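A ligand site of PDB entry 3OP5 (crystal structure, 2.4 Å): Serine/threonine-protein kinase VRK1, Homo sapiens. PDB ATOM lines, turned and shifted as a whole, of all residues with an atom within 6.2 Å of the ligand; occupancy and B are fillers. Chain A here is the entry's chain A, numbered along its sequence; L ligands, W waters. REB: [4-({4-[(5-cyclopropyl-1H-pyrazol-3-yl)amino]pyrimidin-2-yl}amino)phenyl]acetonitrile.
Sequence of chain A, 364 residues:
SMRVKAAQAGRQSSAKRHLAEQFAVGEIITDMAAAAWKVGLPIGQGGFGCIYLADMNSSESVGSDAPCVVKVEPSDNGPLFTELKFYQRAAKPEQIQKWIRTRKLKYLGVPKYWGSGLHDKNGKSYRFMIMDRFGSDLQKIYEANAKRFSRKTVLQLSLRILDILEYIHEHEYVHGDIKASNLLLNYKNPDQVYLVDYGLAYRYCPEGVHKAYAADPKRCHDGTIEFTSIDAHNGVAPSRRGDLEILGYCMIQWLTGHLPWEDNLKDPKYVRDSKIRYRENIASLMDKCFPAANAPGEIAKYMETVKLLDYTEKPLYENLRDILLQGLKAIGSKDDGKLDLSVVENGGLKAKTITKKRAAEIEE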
ATOM      1  N   ILE A  43     -17.003  29.930 -11.211  1.00  0.00           N
ATOM      2  CA  ILE A  43     -15.861  29.104 -11.597  1.00  0.00           C
ATOM      3  C   ILE A  43     -14.901  29.899 -12.514  1.00  0.00           C
ATOM      4  O   ILE A  43     -13.842  29.379 -12.879  1.00  0.00           O
ATOM      5  CB  ILE A  43     -16.292  27.736 -12.215  1.00  0.00           C
ATOM      6  CG1 ILE A  43     -17.316  27.904 -13.360  1.00  0.00           C
ATOM      7  CG2 ILE A  43     -16.808  26.785 -11.127  1.00  0.00           C
ATOM      8  CD1 ILE A  43     -17.378  26.755 -14.327  1.00  0.00           C
ATOM      9  N   GLY A  44     -15.267  31.157 -12.835  1.00  0.00           N
ATOM     10  CA  GLY A  44     -14.473  32.076 -13.649  1.00  0.00           C
ATOM     11  C   GLY A  44     -13.154  32.400 -12.962  1.00  0.00           C
ATOM     12  O   GLY A  44     -13.147  32.983 -11.866  1.00  0.00           O
ATOM     13  N   GLN A  45     -12.040  31.961 -13.569  1.00  0.00           N
ATOM     14  CA  GLN A  45     -10.677  32.099 -13.023  1.00  0.00           C
ATOM     15  C   GLN A  45     -10.064  33.477 -13.288  1.00  0.00           C
ATOM     16  O   GLN A  45      -9.842  33.838 -14.447  1.00  0.00           O
ATOM     17  CB  GLN A  45      -9.757  30.985 -13.591  1.00  0.00           C
ATOM     18  CG  GLN A  45     -10.238  29.556 -13.317  1.00  0.00           C
ATOM     19  CD  GLN A  45      -9.725  28.523 -14.303  1.00  0.00           C
ATOM     20  OE1 GLN A  45      -9.675  28.739 -15.531  1.00  0.00           O
ATOM     21  NE2 GLN A  45      -9.405  27.339 -13.803  1.00  0.00           N
ATOM     22  N   GLY A  46      -9.789  34.216 -12.203  1.00  0.00           N
ATOM     23  CA  GLY A  46      -9.172  35.543 -12.214  1.00  0.00           C
ATOM     24  C   GLY A  46      -9.898  36.596 -13.016  1.00  0.00           C
ATOM     25  O   GLY A  46      -9.409  37.033 -14.061  1.00  0.00           O
ATOM     26  N   PHE A  48      -9.658  36.240 -16.774  1.00  0.00           N
ATOM     27  CA  PHE A  48     -10.718  35.685 -17.613  1.00  0.00           C
ATOM     28  C   PHE A  48     -12.103  36.304 -17.248  1.00  0.00           C
ATOM     29  O   PHE A  48     -12.170  37.206 -16.401  1.00  0.00           O
ATOM     30  CB  PHE A  48     -10.743  34.151 -17.516  1.00  0.00           C
ATOM     31  N   GLY A  49     -13.161  35.836 -17.918  1.00  0.00           N
ATOM     32  CA  GLY A  49     -14.532  36.333 -17.760  1.00  0.00           C
ATOM     33  C   GLY A  49     -15.306  35.931 -16.510  1.00  0.00           C
ATOM     34  O   GLY A  49     -14.777  35.212 -15.638  1.00  0.00           O
ATOM     35  N   ILE A  51     -17.992  33.779 -15.087  1.00  0.00           N
ATOM     36  CA  ILE A  51     -18.620  32.486 -15.380  1.00  0.00           C
ATOM     37  C   ILE A  51     -19.032  31.767 -14.094  1.00  0.00           C
ATOM     38  O   ILE A  51     -18.233  31.652 -13.169  1.00  0.00           O
ATOM     39  CB  ILE A  51     -17.681  31.599 -16.267  1.00  0.00           C
ATOM     40  CG1 ILE A  51     -17.243  32.330 -17.561  1.00  0.00           C
ATOM     41  CG2 ILE A  51     -18.315  30.240 -16.603  1.00  0.00           C
ATOM     42  CD1 ILE A  51     -15.835  32.023 -18.030  1.00  0.00           C
ATOM     43  N   LEU A  53     -21.462  28.115 -12.586  1.00  0.00           N
ATOM     44  CA  LEU A  53     -22.046  26.831 -12.944  1.00  0.00           C
ATOM     45  C   LEU A  53     -23.555  27.066 -13.102  1.00  0.00           C
ATOM     46  O   LEU A  53     -24.104  27.969 -12.454  1.00  0.00           O
ATOM     47  CB  LEU A  53     -21.758  25.749 -11.892  1.00  0.00           C
ATOM     48  CG  LEU A  53     -20.327  25.219 -11.807  1.00  0.00           C
ATOM     49  CD1 LEU A  53     -20.119  24.464 -10.518  1.00  0.00           C
ATOM     50  CD2 LEU A  53     -19.994  24.314 -12.977  1.00  0.00           C
ATOM     51  N   VAL A  69     -22.836  26.077 -17.959  1.00  0.00           N
ATOM     52  CA  VAL A  69     -22.217  27.275 -17.409  1.00  0.00           C
ATOM     53  C   VAL A  69     -22.987  28.501 -17.915  1.00  0.00           C
ATOM     54  O   VAL A  69     -23.540  28.492 -19.016  1.00  0.00           O
ATOM     55  CB  VAL A  69     -20.683  27.437 -17.651  1.00  0.00           C
ATOM     56  CG1 VAL A  69     -19.889  26.328 -16.970  1.00  0.00           C
ATOM     57  CG2 VAL A  69     -20.333  27.573 -19.139  1.00  0.00           C
ATOM     58  N   LYS A  71     -22.250  32.477 -18.808  1.00  0.00           N
ATOM     59  CA  LYS A  71     -21.257  33.521 -19.042  1.00  0.00           C
ATOM     60  C   LYS A  71     -21.979  34.872 -19.003  1.00  0.00           C
ATOM     61  O   LYS A  71     -22.993  35.023 -19.683  1.00  0.00           O
ATOM     62  CB  LYS A  71     -20.531  33.317 -20.379  1.00  0.00           C
ATOM     63  CG  LYS A  71     -19.251  34.141 -20.522  1.00  0.00           C
ATOM     64  CD  LYS A  71     -18.458  33.737 -21.778  1.00  0.00           C
ATOM     65  CE  LYS A  71     -17.368  34.728 -22.114  1.00  0.00           C
ATOM     66  NZ  LYS A  71     -16.137  34.520 -21.313  1.00  0.00           N
ATOM     67  N   GLU A  83     -19.350  36.577 -29.752  1.00  0.00           N
ATOM     68  CA  GLU A  83     -19.424  35.186 -29.308  1.00  0.00           C
ATOM     69  C   GLU A  83     -20.854  34.658 -29.363  1.00  0.00           C
ATOM     70  O   GLU A  83     -21.061  33.545 -29.838  1.00  0.00           O
ATOM     71  CB  GLU A  83     -18.834  35.030 -27.914  1.00  0.00           C
ATOM     72  CG  GLU A  83     -18.589  33.576 -27.546  1.00  0.00           C
ATOM     73  CD  GLU A  83     -17.699  33.357 -26.353  1.00  0.00           C
ATOM     74  OE1 GLU A  83     -17.902  34.043 -25.323  1.00  0.00           O
ATOM     75  OE2 GLU A  83     -16.800  32.477 -26.432  1.00  0.00           O
ATOM     76  N   TYR A  87     -22.438  31.500 -31.761  1.00  0.00           N
ATOM     77  CA  TYR A  87     -23.183  30.399 -31.136  1.00  0.00           C
ATOM     78  C   TYR A  87     -24.635  30.327 -31.644  1.00  0.00           C
ATOM     79  O   TYR A  87     -25.122  29.216 -31.908  1.00  0.00           O
ATOM     80  CB  TYR A  87     -23.155  30.492 -29.603  1.00  0.00           C
ATOM     81  CG  TYR A  87     -21.888  29.915 -28.991  1.00  0.00           C
ATOM     82  CD1 TYR A  87     -20.944  30.743 -28.384  1.00  0.00           C
ATOM     83  CD2 TYR A  87     -21.621  28.555 -29.053  1.00  0.00           C
ATOM     84  CE1 TYR A  87     -19.760  30.214 -27.851  1.00  0.00           C
ATOM     85  CE2 TYR A  87     -20.443  28.029 -28.532  1.00  0.00           C
ATOM     86  CZ  TYR A  87     -19.521  28.857 -27.924  1.00  0.00           C
ATOM     87  OH  TYR A  87     -18.378  28.314 -27.392  1.00  0.00           O
ATOM     88  N   PRO A 111     -18.825  23.776 -28.675  1.00  0.00           N
ATOM     89  CA  PRO A 111     -19.731  23.801 -27.513  1.00  0.00           C
ATOM     90  C   PRO A 111     -21.159  24.159 -27.915  1.00  0.00           C
ATOM     91  O   PRO A 111     -21.343  24.952 -28.827  1.00  0.00           O
ATOM     92  CB  PRO A 111     -19.110  24.863 -26.592  1.00  0.00           C
ATOM     93  CG  PRO A 111     -17.683  25.042 -27.099  1.00  0.00           C
ATOM     94  CD  PRO A 111     -17.802  24.839 -28.578  1.00  0.00           C
ATOM     95  N   MET A 131     -24.133  27.788 -21.904  1.00  0.00           N
ATOM     96  CA  MET A 131     -23.348  26.891 -22.741  1.00  0.00           C
ATOM     97  C   MET A 131     -22.977  25.653 -21.952  1.00  0.00           C
ATOM     98  O   MET A 131     -23.208  25.606 -20.748  1.00  0.00           O
ATOM     99  CB  MET A 131     -22.079  27.594 -23.239  1.00  0.00           C
ATOM    100  CG  MET A 131     -22.319  28.620 -24.332  1.00  0.00           C
ATOM    101  SD  MET A 131     -20.924  29.746 -24.384  1.00  0.00           S
ATOM    102  CE  MET A 131     -21.111  30.606 -22.799  1.00  0.00           C
ATOM    103  N   ASP A 132     -22.398  24.653 -22.652  1.00  0.00           N
ATOM    104  CA  ASP A 132     -21.927  23.393 -22.086  1.00  0.00           C
ATOM    105  C   ASP A 132     -20.837  23.617 -21.044  1.00  0.00           C
ATOM    106  O   ASP A 132     -19.961  24.476 -21.238  1.00  0.00           O
ATOM    107  CB  ASP A 132     -21.351  22.485 -23.190  1.00  0.00           C
ATOM    108  CG  ASP A 132     -22.318  21.826 -24.149  1.00  0.00           C
ATOM    109  OD1 ASP A 132     -23.461  21.532 -23.723  1.00  0.00           O
ATOM    110  OD2 ASP A 132     -21.901  21.507 -25.291  1.00  0.00           O
ATOM    111  N   ARG A 133     -20.866  22.811 -19.987  1.00  0.00           N
ATOM    112  CA  ARG A 133     -19.841  22.811 -18.944  1.00  0.00           C
ATOM    113  C   ARG A 133     -18.743  21.829 -19.379  1.00  0.00           C
ATOM    114  O   ARG A 133     -19.042  20.733 -19.857  1.00  0.00           O
ATOM    115  CB  ARG A 133     -20.446  22.419 -17.585  1.00  0.00           C
ATOM    116  CG  ARG A 133     -19.496  22.599 -16.397  1.00  0.00           C
ATOM    117  CD  ARG A 133     -18.785  21.324 -16.043  1.00  0.00           C
ATOM    118  NE  ARG A 133     -17.953  21.419 -14.846  1.00  0.00           N
ATOM    119  CZ  ARG A 133     -18.364  21.050 -13.638  1.00  0.00           C
ATOM    120  NH1 ARG A 133     -19.627  20.707 -13.439  1.00  0.00           N
ATOM    121  NH2 ARG A 133     -17.517  21.038 -12.624  1.00  0.00           N
ATOM    122  N   PHE A 134     -17.492  22.218 -19.191  1.00  0.00           N
ATOM    123  CA  PHE A 134     -16.360  21.366 -19.539  1.00  0.00           C
ATOM    124  C   PHE A 134     -15.468  21.103 -18.334  1.00  0.00           C
ATOM    125  O   PHE A 134     -15.611  21.743 -17.294  1.00  0.00           O
ATOM    126  CB  PHE A 134     -15.543  21.991 -20.685  1.00  0.00           C
ATOM    127  CG  PHE A 134     -16.317  22.149 -21.966  1.00  0.00           C
ATOM    128  CD1 PHE A 134     -16.896  21.058 -22.589  1.00  0.00           C
ATOM    129  CD2 PHE A 134     -16.488  23.407 -22.539  1.00  0.00           C
ATOM    130  CE1 PHE A 134     -17.651  21.214 -23.745  1.00  0.00           C
ATOM    131  CE2 PHE A 134     -17.221  23.559 -23.705  1.00  0.00           C
ATOM    132  CZ  PHE A 134     -17.798  22.457 -24.300  1.00  0.00           C
ATOM    133  N   GLY A 135     -14.541  20.158 -18.527  1.00  0.00           N
ATOM    134  CA  GLY A 135     -13.525  19.796 -17.549  1.00  0.00           C
ATOM    135  C   GLY A 135     -12.309  20.684 -17.688  1.00  0.00           C
ATOM    136  O   GLY A 135     -12.428  21.887 -17.972  1.00  0.00           O
ATOM    137  N   ASP A 137      -8.757  22.390 -19.106  1.00  0.00           N
ATOM    138  CA  ASP A 137      -8.224  22.878 -20.364  1.00  0.00           C
ATOM    139  C   ASP A 137      -6.933  22.105 -20.606  1.00  0.00           C
ATOM    140  O   ASP A 137      -6.367  21.549 -19.665  1.00  0.00           O
ATOM    141  CB  ASP A 137      -8.015  24.418 -20.351  1.00  0.00           C
ATOM    142  CG  ASP A 137      -6.980  24.945 -19.381  1.00  0.00           C
ATOM    143  OD1 ASP A 137      -5.791  24.645 -19.555  1.00  0.00           O
ATOM    144  OD2 ASP A 137      -7.338  25.754 -18.499  1.00  0.00           O
ATOM    145  N   SER A 181      -4.995  26.355 -24.041  1.00  0.00           N
ATOM    146  CA  SER A 181      -5.859  26.995 -23.046  1.00  0.00           C
ATOM    147  C   SER A 181      -7.296  27.201 -23.559  1.00  0.00           C
ATOM    148  O   SER A 181      -8.204  27.424 -22.745  1.00  0.00           O
ATOM    149  CB  SER A 181      -5.267  28.317 -22.573  1.00  0.00           C
ATOM    150  OG  SER A 181      -5.329  29.329 -23.566  1.00  0.00           O
ATOM    151  N   LEU A 184     -10.803  22.531 -24.120  1.00  0.00           N
ATOM    152  CA  LEU A 184     -11.317  21.969 -22.880  1.00  0.00           C
ATOM    153  C   LEU A 184     -11.883  20.573 -23.097  1.00  0.00           C
ATOM    154  O   LEU A 184     -12.491  20.318 -24.129  1.00  0.00           O
ATOM    155  CB  LEU A 184     -12.393  22.910 -22.298  1.00  0.00           C
ATOM    156  CG  LEU A 184     -11.904  24.076 -21.414  1.00  0.00           C
ATOM    157  CD1 LEU A 184     -11.167  25.146 -22.216  1.00  0.00           C
ATOM    158  CD2 LEU A 184     -13.064  24.734 -20.696  1.00  0.00           C
ATOM    159  N   VAL A 196     -13.047  26.419 -27.459  1.00  0.00           N
ATOM    160  CA  VAL A 196     -13.825  27.499 -26.858  1.00  0.00           C
ATOM    161  C   VAL A 196     -13.254  28.864 -27.274  1.00  0.00           C
ATOM    162  O   VAL A 196     -12.219  28.921 -27.952  1.00  0.00           O
ATOM    163  CB  VAL A 196     -13.951  27.371 -25.308  1.00  0.00           C
ATOM    164  CG1 VAL A 196     -14.585  26.037 -24.905  1.00  0.00           C
ATOM    165  CG2 VAL A 196     -12.612  27.578 -24.593  1.00  0.00           C
ATOM    166  N   ASP A 197     -13.926  29.963 -26.850  1.00  0.00           N
ATOM    167  CA  ASP A 197     -13.609  31.376 -27.048  1.00  0.00           C
ATOM    168  C   ASP A 197     -13.826  31.818 -28.508  1.00  0.00           C
ATOM    169  O   ASP A 197     -12.929  31.686 -29.360  1.00  0.00           O
ATOM    170  CB  ASP A 197     -12.185  31.728 -26.565  1.00  0.00           C
ATOM    171  CG  ASP A 197     -11.927  33.212 -26.342  1.00  0.00           C
ATOM    172  OD1 ASP A 197     -12.736  34.047 -26.803  1.00  0.00           O
ATOM    173  OD2 ASP A 197     -10.887  33.541 -25.720  1.00  0.00           O
HETATM  174  C10 REB L   1     -15.875  26.925 -18.896  1.00  0.00           C
HETATM  175  N12 REB L   1     -16.146  25.347 -17.493  1.00  0.00           N
HETATM  176  C15 REB L   1     -14.490  28.148 -15.794  1.00  0.00           C
HETATM  177  C20 REB L   1     -12.958  31.166 -19.991  1.00  0.00           C
HETATM  178  C21 REB L   1     -12.246  30.048 -19.506  1.00  0.00           C
HETATM  179  C22 REB L   1     -12.548  28.675 -20.015  1.00  0.00           C
HETATM  180  C24 REB L   1     -11.184  30.417 -18.474  1.00  0.00           C
HETATM  181  C02 REB L   1     -18.291  26.832 -22.949  1.00  0.00           C
HETATM  182  C03 REB L   1     -18.095  27.835 -23.908  1.00  0.00           C
HETATM  183  N04 REB L   1     -17.098  28.827 -23.713  1.00  0.00           N
HETATM  184  C05 REB L   1     -16.355  28.876 -22.646  1.00  0.00           C
HETATM  185  N06 REB L   1     -16.589  27.901 -21.688  1.00  0.00           N
HETATM  186  C07 REB L   1     -17.501  26.899 -21.780  1.00  0.00           C
HETATM  187  N08 REB L   1     -17.497  25.996 -20.625  1.00  0.00           N
HETATM  188  C09 REB L   1     -16.821  25.948 -19.410  1.00  0.00           C
HETATM  189  C11 REB L   1     -15.509  26.445 -17.676  1.00  0.00           C
HETATM  190  N13 REB L   1     -16.954  25.028 -18.523  1.00  0.00           N
HETATM  191  C14 REB L   1     -14.596  26.968 -16.661  1.00  0.00           C
HETATM  192  C16 REB L   1     -13.498  27.938 -16.895  1.00  0.00           C
HETATM  193  N17 REB L   1     -15.371  29.759 -22.368  1.00  0.00           N
HETATM  194  C18 REB L   1     -14.302  29.785 -21.435  1.00  0.00           C
HETATM  195  C19 REB L   1     -13.972  31.033 -20.950  1.00  0.00           C
HETATM  196  C23 REB L   1     -13.624  28.579 -21.002  1.00  0.00           C
HETATM  197  C25 REB L   1     -11.895  30.866 -17.259  1.00  0.00           C
HETATM  198  N26 REB L   1     -12.514  31.358 -16.439  1.00  0.00           N
HETATM  199  O   HOH W   1     -12.291  26.835 -13.528  1.00  0.00           O
HETATM  200  O   HOH W   2      -9.163  28.356 -20.512  1.00  0.00           O
HETATM  201  O   HOH W   3     -16.652  29.830 -26.069  1.00  0.00           O
HETATM  202  O   HOH W   4     -15.305  31.978 -24.086  1.00  0.00           O
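Ile 43 touches the ligand. CA of Gly 44 touches N26 of the ligand (3.5 Å). Phe 48 touches the ligand (CB to N26, 3.5 Å). Ile 51 touches the ligand (CD1 to C20, 3.6 Å). CG1 of Val 69 touches N13 of the ligand (3.6 Å). Tyr 87 touches the ligand. Met 131 touches the ligand. CA of Arg 133 touches N13 of the ligand, at 3.7 Å. Leu 184 touches the ligand (CD2 to C23, 3.9 Å). Val 196 touches the ligand (CB to N04, 3.8 Å). Along chain A the residues within 4 Å of the ligand span positions 43 to 196. The nearest printed residue that does not touch the ligand is Lys 71 (4.1 Å).
Water W3 lies within hydrogen-bond range of a nitrogen (N04) of the ligand, the side-chain hydroxyl of Tyr 87, the side-chain carboxylate of Glu 83 and the backbone NH of Asp 197. Water W4 lies within hydrogen-bond range of a nitrogen (N17) of the ligand (2.8 Å) and the side-chain carboxylate of Glu 83 (2.8 Å). Water W1 bridges the side-chain amide nitrogen (NE2) of Gln 45 and the backbone carbonyl oxygen (O) of Ile 43.
N of Val 69 lies within hydrogen-bond range of O of Met 131. The backbone carbonyl oxygen of Ile 51 lies within hydrogen-bond range of the backbone NH of Ile 43 (2.9 Å). The backbone NH (N) of Gly 44 sits at hydrogen-bond distance from the backbone carbonyl oxygen (O) of Ile 51 (3.0 Å).
The backbone NH of Gln 45 lies within hydrogen-bond range of a nitrogen (N26) of the ligand, at 3.0 Å. O of Asp 132 lies within hydrogen-bond range of N08 of the ligand, at 3.0 Å. A nitrogen (N13) of the ligand is in hydrogen-bond range of the backbone NH (N) of Phe 134, 2.9 Å away.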
